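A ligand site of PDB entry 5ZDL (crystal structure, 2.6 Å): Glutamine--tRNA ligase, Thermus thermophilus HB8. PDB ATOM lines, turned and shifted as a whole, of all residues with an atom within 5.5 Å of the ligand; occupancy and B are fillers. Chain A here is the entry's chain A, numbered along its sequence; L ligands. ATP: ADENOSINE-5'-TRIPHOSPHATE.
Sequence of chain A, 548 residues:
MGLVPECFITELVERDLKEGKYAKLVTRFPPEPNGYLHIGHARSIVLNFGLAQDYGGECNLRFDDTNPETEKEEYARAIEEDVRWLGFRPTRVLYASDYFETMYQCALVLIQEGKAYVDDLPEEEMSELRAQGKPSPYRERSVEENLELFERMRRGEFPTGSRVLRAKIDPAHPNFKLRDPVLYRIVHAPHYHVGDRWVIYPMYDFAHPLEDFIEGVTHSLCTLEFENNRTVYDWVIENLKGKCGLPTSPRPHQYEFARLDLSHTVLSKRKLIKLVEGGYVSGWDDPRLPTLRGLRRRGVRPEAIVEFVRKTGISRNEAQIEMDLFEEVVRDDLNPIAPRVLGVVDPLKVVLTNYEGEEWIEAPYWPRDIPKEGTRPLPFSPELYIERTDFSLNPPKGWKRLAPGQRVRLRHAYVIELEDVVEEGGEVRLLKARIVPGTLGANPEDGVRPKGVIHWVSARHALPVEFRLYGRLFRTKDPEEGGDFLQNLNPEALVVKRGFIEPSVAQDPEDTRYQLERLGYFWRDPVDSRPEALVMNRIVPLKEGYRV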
ATOM      1  N   ARG A  28       0.480 -28.368  -6.754  1.00  0.00           N
ATOM      2  CA  ARG A  28      -0.023 -29.084  -7.893  1.00  0.00           C
ATOM      3  C   ARG A  28       0.124 -28.300  -9.154  1.00  0.00           C
ATOM      4  O   ARG A  28       0.153 -27.121  -9.117  1.00  0.00           O
ATOM      5  CB  ARG A  28      -1.504 -29.374  -7.690  1.00  0.00           C
ATOM      6  CG  ARG A  28      -2.438 -28.277  -8.126  1.00  0.00           C
ATOM      7  CD  ARG A  28      -2.550 -27.151  -7.128  1.00  0.00           C
ATOM      8  NE  ARG A  28      -3.500 -26.148  -7.522  1.00  0.00           N
ATOM      9  CZ  ARG A  28      -3.188 -25.041  -8.171  1.00  0.00           C
ATOM     10  NH1 ARG A  28      -1.962 -24.829  -8.553  1.00  0.00           N
ATOM     11  NH2 ARG A  28      -4.094 -24.161  -8.456  1.00  0.00           N
ATOM     12  N   PHE A  29       0.241 -28.963 -10.288  1.00  0.00           N
ATOM     13  CA  PHE A  29       0.220 -28.291 -11.551  1.00  0.00           C
ATOM     14  C   PHE A  29      -1.068 -28.822 -12.114  1.00  0.00           C
ATOM     15  O   PHE A  29      -1.213 -30.006 -12.285  1.00  0.00           O
ATOM     16  CB  PHE A  29       1.401 -28.637 -12.417  1.00  0.00           C
ATOM     17  CG  PHE A  29       1.318 -28.081 -13.798  1.00  0.00           C
ATOM     18  CD1 PHE A  29       1.095 -26.759 -14.020  1.00  0.00           C
ATOM     19  CD2 PHE A  29       1.478 -28.904 -14.888  1.00  0.00           C
ATOM     20  CE1 PHE A  29       1.022 -26.256 -15.282  1.00  0.00           C
ATOM     21  CE2 PHE A  29       1.406 -28.415 -16.155  1.00  0.00           C
ATOM     22  CZ  PHE A  29       1.180 -27.085 -16.356  1.00  0.00           C
ATOM     23  N   PRO A  30      -1.999 -27.965 -12.462  1.00  0.00           N
ATOM     24  CA  PRO A  30      -3.315 -28.418 -12.855  1.00  0.00           C
ATOM     25  C   PRO A  30      -3.869 -27.891 -14.152  1.00  0.00           C
ATOM     26  O   PRO A  30      -4.809 -27.143 -14.181  1.00  0.00           O
ATOM     27  CB  PRO A  30      -4.143 -27.904 -11.704  1.00  0.00           C
ATOM     28  CG  PRO A  30      -3.509 -26.608 -11.419  1.00  0.00           C
ATOM     29  CD  PRO A  30      -2.088 -26.654 -11.840  1.00  0.00           C
ATOM     30  N   PRO A  31      -3.282 -28.323 -15.228  1.00  0.00           N
ATOM     31  CA  PRO A  31      -3.708 -27.925 -16.549  1.00  0.00           C
ATOM     32  C   PRO A  31      -4.900 -28.686 -17.038  1.00  0.00           C
ATOM     33  O   PRO A  31      -5.178 -29.753 -16.587  1.00  0.00           O
ATOM     34  CB  PRO A  31      -2.519 -28.303 -17.389  1.00  0.00           C
ATOM     35  CG  PRO A  31      -2.024 -29.514 -16.742  1.00  0.00           C
ATOM     36  CD  PRO A  31      -2.175 -29.270 -15.295  1.00  0.00           C
ATOM     37  N   GLU A  32      -5.631 -28.080 -17.949  1.00  0.00           N
ATOM     38  CA  GLU A  32      -6.751 -28.739 -18.574  1.00  0.00           C
ATOM     39  C   GLU A  32      -6.196 -29.484 -19.747  1.00  0.00           C
ATOM     40  O   GLU A  32      -5.366 -28.969 -20.479  1.00  0.00           O
ATOM     41  CB  GLU A  32      -7.756 -27.729 -19.012  1.00  0.00           C
ATOM     42  CG  GLU A  32      -8.986 -28.353 -19.641  1.00  0.00           C
ATOM     43  CD  GLU A  32     -10.089 -27.335 -19.871  1.00  0.00           C
ATOM     44  OE1 GLU A  32      -9.888 -26.124 -19.568  1.00  0.00           O
ATOM     45  OE2 GLU A  32     -11.156 -27.769 -20.349  1.00  0.00           O
ATOM     46  N   ASN A  34      -6.898 -30.009 -22.863  1.00  0.00           N
ATOM     47  CA  ASN A  34      -7.609 -29.611 -24.098  1.00  0.00           C
ATOM     48  C   ASN A  34      -6.701 -28.885 -25.073  1.00  0.00           C
ATOM     49  O   ASN A  34      -7.151 -28.233 -26.035  1.00  0.00           O
ATOM     50  CB  ASN A  34      -8.788 -28.722 -23.751  1.00  0.00           C
ATOM     51  CG  ASN A  34      -8.362 -27.488 -22.996  1.00  0.00           C
ATOM     52  OD1 ASN A  34      -7.376 -27.510 -22.253  1.00  0.00           O
ATOM     53  ND2 ASN A  34      -9.104 -26.409 -23.171  1.00  0.00           N
ATOM     54  N   LEU A  37       0.982 -27.800 -24.053  1.00  0.00           N
ATOM     55  CA  LEU A  37       1.592 -26.800 -23.205  1.00  0.00           C
ATOM     56  C   LEU A  37       2.505 -25.864 -23.996  1.00  0.00           C
ATOM     57  O   LEU A  37       3.128 -26.258 -24.951  1.00  0.00           O
ATOM     58  CB  LEU A  37       2.318 -27.484 -22.074  1.00  0.00           C
ATOM     59  CG  LEU A  37       1.393 -28.249 -21.155  1.00  0.00           C
ATOM     60  CD1 LEU A  37       2.275 -29.041 -20.199  1.00  0.00           C
ATOM     61  CD2 LEU A  37       0.452 -27.357 -20.361  1.00  0.00           C
ATOM     62  N   HIS A  38       2.501 -24.591 -23.620  1.00  0.00           N
ATOM     63  CA  HIS A  38       3.472 -23.642 -24.108  1.00  0.00           C
ATOM     64  C   HIS A  38       4.516 -23.300 -23.044  1.00  0.00           C
ATOM     65  O   HIS A  38       4.472 -23.794 -21.934  1.00  0.00           O
ATOM     66  CB  HIS A  38       2.774 -22.395 -24.692  1.00  0.00           C
ATOM     67  CG  HIS A  38       1.849 -21.680 -23.753  1.00  0.00           C
ATOM     68  ND1 HIS A  38       2.242 -21.173 -22.538  1.00  0.00           N
ATOM     69  CD2 HIS A  38       0.549 -21.326 -23.900  1.00  0.00           C
ATOM     70  CE1 HIS A  38       1.224 -20.575 -21.954  1.00  0.00           C
ATOM     71  NE2 HIS A  38       0.184 -20.644 -22.760  1.00  0.00           N
ATOM     72  N   GLY A  40       4.860 -20.456 -21.459  1.00  0.00           N
ATOM     73  CA  GLY A  40       4.153 -19.959 -20.270  1.00  0.00           C
ATOM     74  C   GLY A  40       3.928 -20.999 -19.179  1.00  0.00           C
ATOM     75  O   GLY A  40       4.300 -20.800 -18.032  1.00  0.00           O
ATOM     76  N   HIS A  41       3.329 -22.137 -19.535  1.00  0.00           N
ATOM     77  CA  HIS A  41       3.074 -23.219 -18.553  1.00  0.00           C
ATOM     78  C   HIS A  41       4.360 -23.700 -17.887  1.00  0.00           C
ATOM     79  O   HIS A  41       4.317 -24.207 -16.783  1.00  0.00           O
ATOM     80  CB  HIS A  41       2.365 -24.437 -19.183  1.00  0.00           C
ATOM     81  CG  HIS A  41       1.063 -24.133 -19.846  1.00  0.00           C
ATOM     82  ND1 HIS A  41       0.943 -24.041 -21.208  1.00  0.00           N
ATOM     83  CD2 HIS A  41      -0.170 -23.887 -19.334  1.00  0.00           C
ATOM     84  CE1 HIS A  41      -0.304 -23.731 -21.527  1.00  0.00           C
ATOM     85  NE2 HIS A  41      -0.999 -23.632 -20.406  1.00  0.00           N
ATOM     86  N   ARG A  43       6.519 -21.833 -16.552  1.00  0.00           N
ATOM     87  CA  ARG A  43       6.677 -21.065 -15.308  1.00  0.00           C
ATOM     88  C   ARG A  43       5.936 -21.744 -14.144  1.00  0.00           C
ATOM     89  O   ARG A  43       6.502 -21.932 -13.075  1.00  0.00           O
ATOM     90  CB  ARG A  43       6.238 -19.611 -15.500  1.00  0.00           C
ATOM     91  CG  ARG A  43       6.287 -18.764 -14.236  1.00  0.00           C
ATOM     92  CD  ARG A  43       6.014 -17.301 -14.573  1.00  0.00           C
ATOM     93  NE  ARG A  43       7.224 -16.624 -15.038  1.00  0.00           N
ATOM     94  CZ  ARG A  43       7.276 -15.358 -15.420  1.00  0.00           C
ATOM     95  NH1 ARG A  43       6.208 -14.567 -15.415  1.00  0.00           N
ATOM     96  NH2 ARG A  43       8.441 -14.861 -15.800  1.00  0.00           N
ATOM     97  N   SER A  44       4.692 -22.143 -14.378  1.00  0.00           N
ATOM     98  CA  SER A  44       3.920 -22.847 -13.367  1.00  0.00           C
ATOM     99  C   SER A  44       4.526 -24.206 -13.011  1.00  0.00           C
ATOM    100  O   SER A  44       4.536 -24.608 -11.838  1.00  0.00           O
ATOM    101  CB  SER A  44       2.476 -23.041 -13.815  1.00  0.00           C
ATOM    102  OG  SER A  44       1.643 -23.164 -12.684  1.00  0.00           O
ATOM    103  N   LEU A 221      -1.011 -22.360  -6.192  1.00  0.00           N
ATOM    104  CA  LEU A 221      -0.410 -21.272  -6.979  1.00  0.00           C
ATOM    105  C   LEU A 221      -0.958 -21.202  -8.406  1.00  0.00           C
ATOM    106  O   LEU A 221      -0.901 -22.174  -9.182  1.00  0.00           O
ATOM    107  CB  LEU A 221       1.118 -21.428  -7.026  1.00  0.00           C
ATOM    108  CG  LEU A 221       1.794 -21.696  -5.682  1.00  0.00           C
ATOM    109  CD1 LEU A 221       3.294 -21.742  -5.859  1.00  0.00           C
ATOM    110  CD2 LEU A 221       1.421 -20.653  -4.633  1.00  0.00           C
ATOM    111  N   CYS A 222      -1.485 -20.041  -8.733  1.00  0.00           N
ATOM    112  CA  CYS A 222      -2.069 -19.755 -10.036  1.00  0.00           C
ATOM    113  C   CYS A 222      -1.734 -18.313 -10.431  1.00  0.00           C
ATOM    114  O   CYS A 222      -1.227 -17.539  -9.618  1.00  0.00           O
ATOM    115  CB  CYS A 222      -3.573 -19.970  -9.969  1.00  0.00           C
ATOM    116  SG  CYS A 222      -4.217 -19.340  -8.411  1.00  0.00           S
ATOM    117  N   THR A 223      -2.027 -17.961 -11.680  1.00  0.00           N
ATOM    118  CA  THR A 223      -1.673 -16.672 -12.226  1.00  0.00           C
ATOM    119  C   THR A 223      -2.729 -15.635 -11.858  1.00  0.00           C
ATOM    120  O   THR A 223      -3.841 -16.010 -11.454  1.00  0.00           O
ATOM    121  CB  THR A 223      -1.623 -16.710 -13.745  1.00  0.00           C
ATOM    122  OG1 THR A 223      -2.928 -17.032 -14.222  1.00  0.00           O
ATOM    123  CG2 THR A 223      -0.627 -17.724 -14.258  1.00  0.00           C
ATOM    124  N   GLU A 225      -4.924 -13.820 -13.257  1.00  0.00           N
ATOM    125  CA  GLU A 225      -6.281 -13.757 -13.810  1.00  0.00           C
ATOM    126  C   GLU A 225      -7.306 -14.134 -12.728  1.00  0.00           C
ATOM    127  O   GLU A 225      -8.408 -13.561 -12.657  1.00  0.00           O
ATOM    128  CB  GLU A 225      -6.426 -14.665 -15.045  1.00  0.00           C
ATOM    129  CG  GLU A 225      -5.641 -14.179 -16.254  1.00  0.00           C
ATOM    130  CD  GLU A 225      -5.234 -15.322 -17.180  1.00  0.00           C
ATOM    131  OE1 GLU A 225      -6.097 -16.164 -17.504  1.00  0.00           O
ATOM    132  OE2 GLU A 225      -4.039 -15.369 -17.581  1.00  0.00           O
ATOM    133  N   PHE A 257       0.669 -15.269  -8.956  1.00  0.00           N
ATOM    134  CA  PHE A 257       1.942 -14.795  -9.478  1.00  0.00           C
ATOM    135  C   PHE A 257       1.723 -14.331 -10.929  1.00  0.00           C
ATOM    136  O   PHE A 257       0.665 -14.546 -11.501  1.00  0.00           O
ATOM    137  CB  PHE A 257       3.001 -15.905  -9.385  1.00  0.00           C
ATOM    138  CG  PHE A 257       2.733 -17.059 -10.272  1.00  0.00           C
ATOM    139  CD1 PHE A 257       1.887 -18.052  -9.875  1.00  0.00           C
ATOM    140  CD2 PHE A 257       3.289 -17.118 -11.531  1.00  0.00           C
ATOM    141  CE1 PHE A 257       1.618 -19.109 -10.718  1.00  0.00           C
ATOM    142  CE2 PHE A 257       3.029 -18.173 -12.378  1.00  0.00           C
ATOM    143  CZ  PHE A 257       2.192 -19.179 -11.965  1.00  0.00           C
ATOM    144  N   ALA A 258       2.734 -13.696 -11.504  1.00  0.00           N
ATOM    145  CA  ALA A 258       2.546 -13.074 -12.813  1.00  0.00           C
ATOM    146  C   ALA A 258       2.703 -14.042 -13.979  1.00  0.00           C
ATOM    147  O   ALA A 258       3.745 -14.689 -14.121  1.00  0.00           O
ATOM    148  CB  ALA A 258       3.465 -11.873 -12.978  1.00  0.00           C
ATOM    149  N   ARG A 259       1.645 -14.102 -14.772  1.00  0.00           N
ATOM    150  CA  ARG A 259       1.599 -14.653 -16.132  1.00  0.00           C
ATOM    151  C   ARG A 259       2.820 -14.270 -16.955  1.00  0.00           C
ATOM    152  O   ARG A 259       3.209 -13.123 -16.956  1.00  0.00           O
ATOM    153  CB  ARG A 259       0.327 -14.086 -16.824  1.00  0.00           C
ATOM    154  CG  ARG A 259      -0.269 -14.881 -17.985  1.00  0.00           C
ATOM    155  CD  ARG A 259      -1.385 -14.125 -18.735  1.00  0.00           C
ATOM    156  NE  ARG A 259      -0.843 -12.974 -19.475  1.00  0.00           N
ATOM    157  CZ  ARG A 259      -0.190 -13.039 -20.646  1.00  0.00           C
ATOM    158  NH1 ARG A 259       0.036 -14.209 -21.248  1.00  0.00           N
ATOM    159  NH2 ARG A 259       0.260 -11.927 -21.215  1.00  0.00           N
ATOM    160  N   LEU A 260       3.436 -15.220 -17.653  1.00  0.00           N
ATOM    161  CA  LEU A 260       4.507 -14.878 -18.579  1.00  0.00           C
ATOM    162  C   LEU A 260       3.940 -14.452 -19.949  1.00  0.00           C
ATOM    163  O   LEU A 260       2.959 -15.017 -20.471  1.00  0.00           O
ATOM    164  CB  LEU A 260       5.510 -16.021 -18.721  1.00  0.00           C
ATOM    165  CG  LEU A 260       6.517 -15.873 -19.878  1.00  0.00           C
ATOM    166  CD1 LEU A 260       7.463 -14.695 -19.628  1.00  0.00           C
ATOM    167  CD2 LEU A 260       7.305 -17.149 -20.088  1.00  0.00           C
ATOM    168  N   ASP A 261       4.602 -13.438 -20.518  1.00  0.00           N
ATOM    169  CA  ASP A 261       4.155 -12.715 -21.683  1.00  0.00           C
ATOM    170  C   ASP A 261       5.449 -12.444 -22.425  1.00  0.00           C
ATOM    171  O   ASP A 261       6.317 -11.728 -21.931  1.00  0.00           O
ATOM    172  CB  ASP A 261       3.500 -11.418 -21.199  1.00  0.00           C
ATOM    173  CG  ASP A 261       3.240 -10.419 -22.314  1.00  0.00           C
ATOM    174  OD1 ASP A 261       3.244 -10.796 -23.510  1.00  0.00           O
ATOM    175  OD2 ASP A 261       3.034  -9.216 -21.972  1.00  0.00           O
ATOM    176  N   LEU A 267       0.638 -16.593 -26.949  1.00  0.00           N
ATOM    177  CA  LEU A 267       0.313 -17.794 -26.176  1.00  0.00           C
ATOM    178  C   LEU A 267      -1.200 -18.042 -25.948  1.00  0.00           C
ATOM    179  O   LEU A 267      -1.598 -19.121 -25.496  1.00  0.00           O
ATOM    180  CB  LEU A 267       1.037 -17.711 -24.831  1.00  0.00           C
ATOM    181  CG  LEU A 267       2.551 -17.434 -24.921  1.00  0.00           C
ATOM    182  CD1 LEU A 267       3.103 -17.078 -23.552  1.00  0.00           C
ATOM    183  CD2 LEU A 267       3.305 -18.612 -25.525  1.00  0.00           C
ATOM    184  N   LYS A 269      -4.507 -19.379 -26.477  1.00  0.00           N
ATOM    185  CA  LYS A 269      -4.872 -20.596 -27.191  1.00  0.00           C
ATOM    186  C   LYS A 269      -5.600 -20.251 -28.487  1.00  0.00           C
ATOM    187  O   LYS A 269      -5.190 -20.697 -29.564  1.00  0.00           O
ATOM    188  CB  LYS A 269      -5.724 -21.519 -26.309  1.00  0.00           C
ATOM    189  CG  LYS A 269      -5.698 -22.979 -26.749  1.00  0.00           C
ATOM    190  CD  LYS A 269      -7.082 -23.612 -26.766  1.00  0.00           C
ATOM    191  CE  LYS A 269      -7.677 -23.787 -25.361  1.00  0.00           C
ATOM    192  NZ  LYS A 269      -9.089 -24.275 -25.419  1.00  0.00           N
HETATM  193  PB  ATP L   1      -4.949 -21.822 -19.450  1.00  0.00           P
HETATM  194  O1B ATP L   1      -5.544 -20.506 -18.679  1.00  0.00           O
HETATM  195  O2B ATP L   1      -3.568 -21.478 -19.942  1.00  0.00           O
HETATM  196  O3B ATP L   1      -5.965 -22.293 -20.492  1.00  0.00           O
HETATM  197  PA  ATP L   1      -4.185 -24.405 -18.429  1.00  0.00           P
HETATM  198  O1A ATP L   1      -5.094 -25.393 -17.776  1.00  0.00           O
HETATM  199  O2A ATP L   1      -3.866 -24.697 -19.874  1.00  0.00           O
HETATM  200  O3A ATP L   1      -4.876 -22.935 -18.259  1.00  0.00           O
HETATM  201  O5' ATP L   1      -2.818 -24.200 -17.605  1.00  0.00           O
HETATM  202  C5' ATP L   1      -2.693 -24.633 -16.244  1.00  0.00           C
HETATM  203  C4' ATP L   1      -1.989 -23.630 -15.336  1.00  0.00           C
HETATM  204  O4' ATP L   1      -0.861 -23.054 -15.978  1.00  0.00           O
HETATM  205  C3' ATP L   1      -2.927 -22.500 -14.938  1.00  0.00           C
HETATM  206  O3' ATP L   1      -3.393 -22.611 -13.587  1.00  0.00           O
HETATM  207  C2' ATP L   1      -2.107 -21.248 -15.048  1.00  0.00           C
HETATM  208  O2' ATP L   1      -2.099 -20.625 -13.760  1.00  0.00           O
HETATM  209  C1' ATP L   1      -0.739 -21.687 -15.576  1.00  0.00           C
HETATM  210  N9  ATP L   1      -0.358 -20.842 -16.738  1.00  0.00           N
HETATM  211  C8  ATP L   1      -1.051 -20.757 -17.887  1.00  0.00           C
HETATM  212  N7  ATP L   1      -0.456 -19.879 -18.739  1.00  0.00           N
HETATM  213  C5  ATP L   1       0.619 -19.385 -18.142  1.00  0.00           C
HETATM  214  C6  ATP L   1       1.667 -18.429 -18.484  1.00  0.00           C
HETATM  215  N6  ATP L   1       1.654 -17.824 -19.690  1.00  0.00           N
HETATM  216  N1  ATP L   1       2.637 -18.175 -17.572  1.00  0.00           N
HETATM  217  C2  ATP L   1       2.651 -18.780 -16.365  1.00  0.00           C
HETATM  218  N3  ATP L   1       1.718 -19.677 -15.988  1.00  0.00           N
HETATM  219  C4  ATP L   1       0.693 -20.011 -16.815  1.00  0.00           C
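The backbone NH of Glu 32 is in hydrogen-bond range of an oxygen (O1A) of the ligand, at 2.7 Å.
N of Leu 260 is in hydrogen-bond range of N1 of the ligand (3.1 Å).
A nitrogen (N6) of the ligand lies within hydrogen-bond range of the backbone carbonyl oxygen (O) of Leu 260 (3.2 Å).
A ring nitrogen (NE2) of His 41 lies within hydrogen-bond range of an oxygen (O2A) of the ligand, 3.1 Å away.
The backbone NH of Thr 223 lies close to an oxygen (O2') of the ligand, 3.4 Å away.
The backbone carbonyl oxygen (O) of Glu 32 lies close to the side-chain amide oxygen (OD1) of Asn 34.
The backbone NH (N) of Gly 40 lies within hydrogen-bond range of a ring nitrogen (ND1) of His 38 (2.9 Å).
The backbone NH (N) of His 38 sits at hydrogen-bond distance from a ring nitrogen (ND1) of His 41 (2.9 Å).
The guanidinium group (NH1) of Arg 43 lies within hydrogen-bond range of the backbone carbonyl oxygen (O) of Ala 258.
The backbone carbonyl oxygen (O) of Cys 222 is in hydrogen-bond range of the backbone NH (N) of Phe 257.
The guanidinium group (NH2) of Arg 259 is in salt-bridge range of the side-chain carboxylate (OD1) of Asp 261, 3.9 Å away.
O of Gly 40 lies close to N1 of the ligand (3.1 Å).
Phe 29 touches the ligand (CE1 to O4', 3.8 Å).
O of Pro 30 touches C5' of the ligand, at 3.9 Å.
Pro 31 touches the ligand.
His 38 touches the ligand (CE1 to N6, 3.6 Å).
Arg 43 touches the ligand (CB to C2, 3.8 Å).
CB of Ser 44 touches C1' of the ligand (3.9 Å).
Cys 222 touches the ligand.
Arg 259 touches the ligand.
Hydrophobic or aromatic side chains within 4 Å of the ligand: Phe 29, Pro 31, His 38, His 41 and Leu 260.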
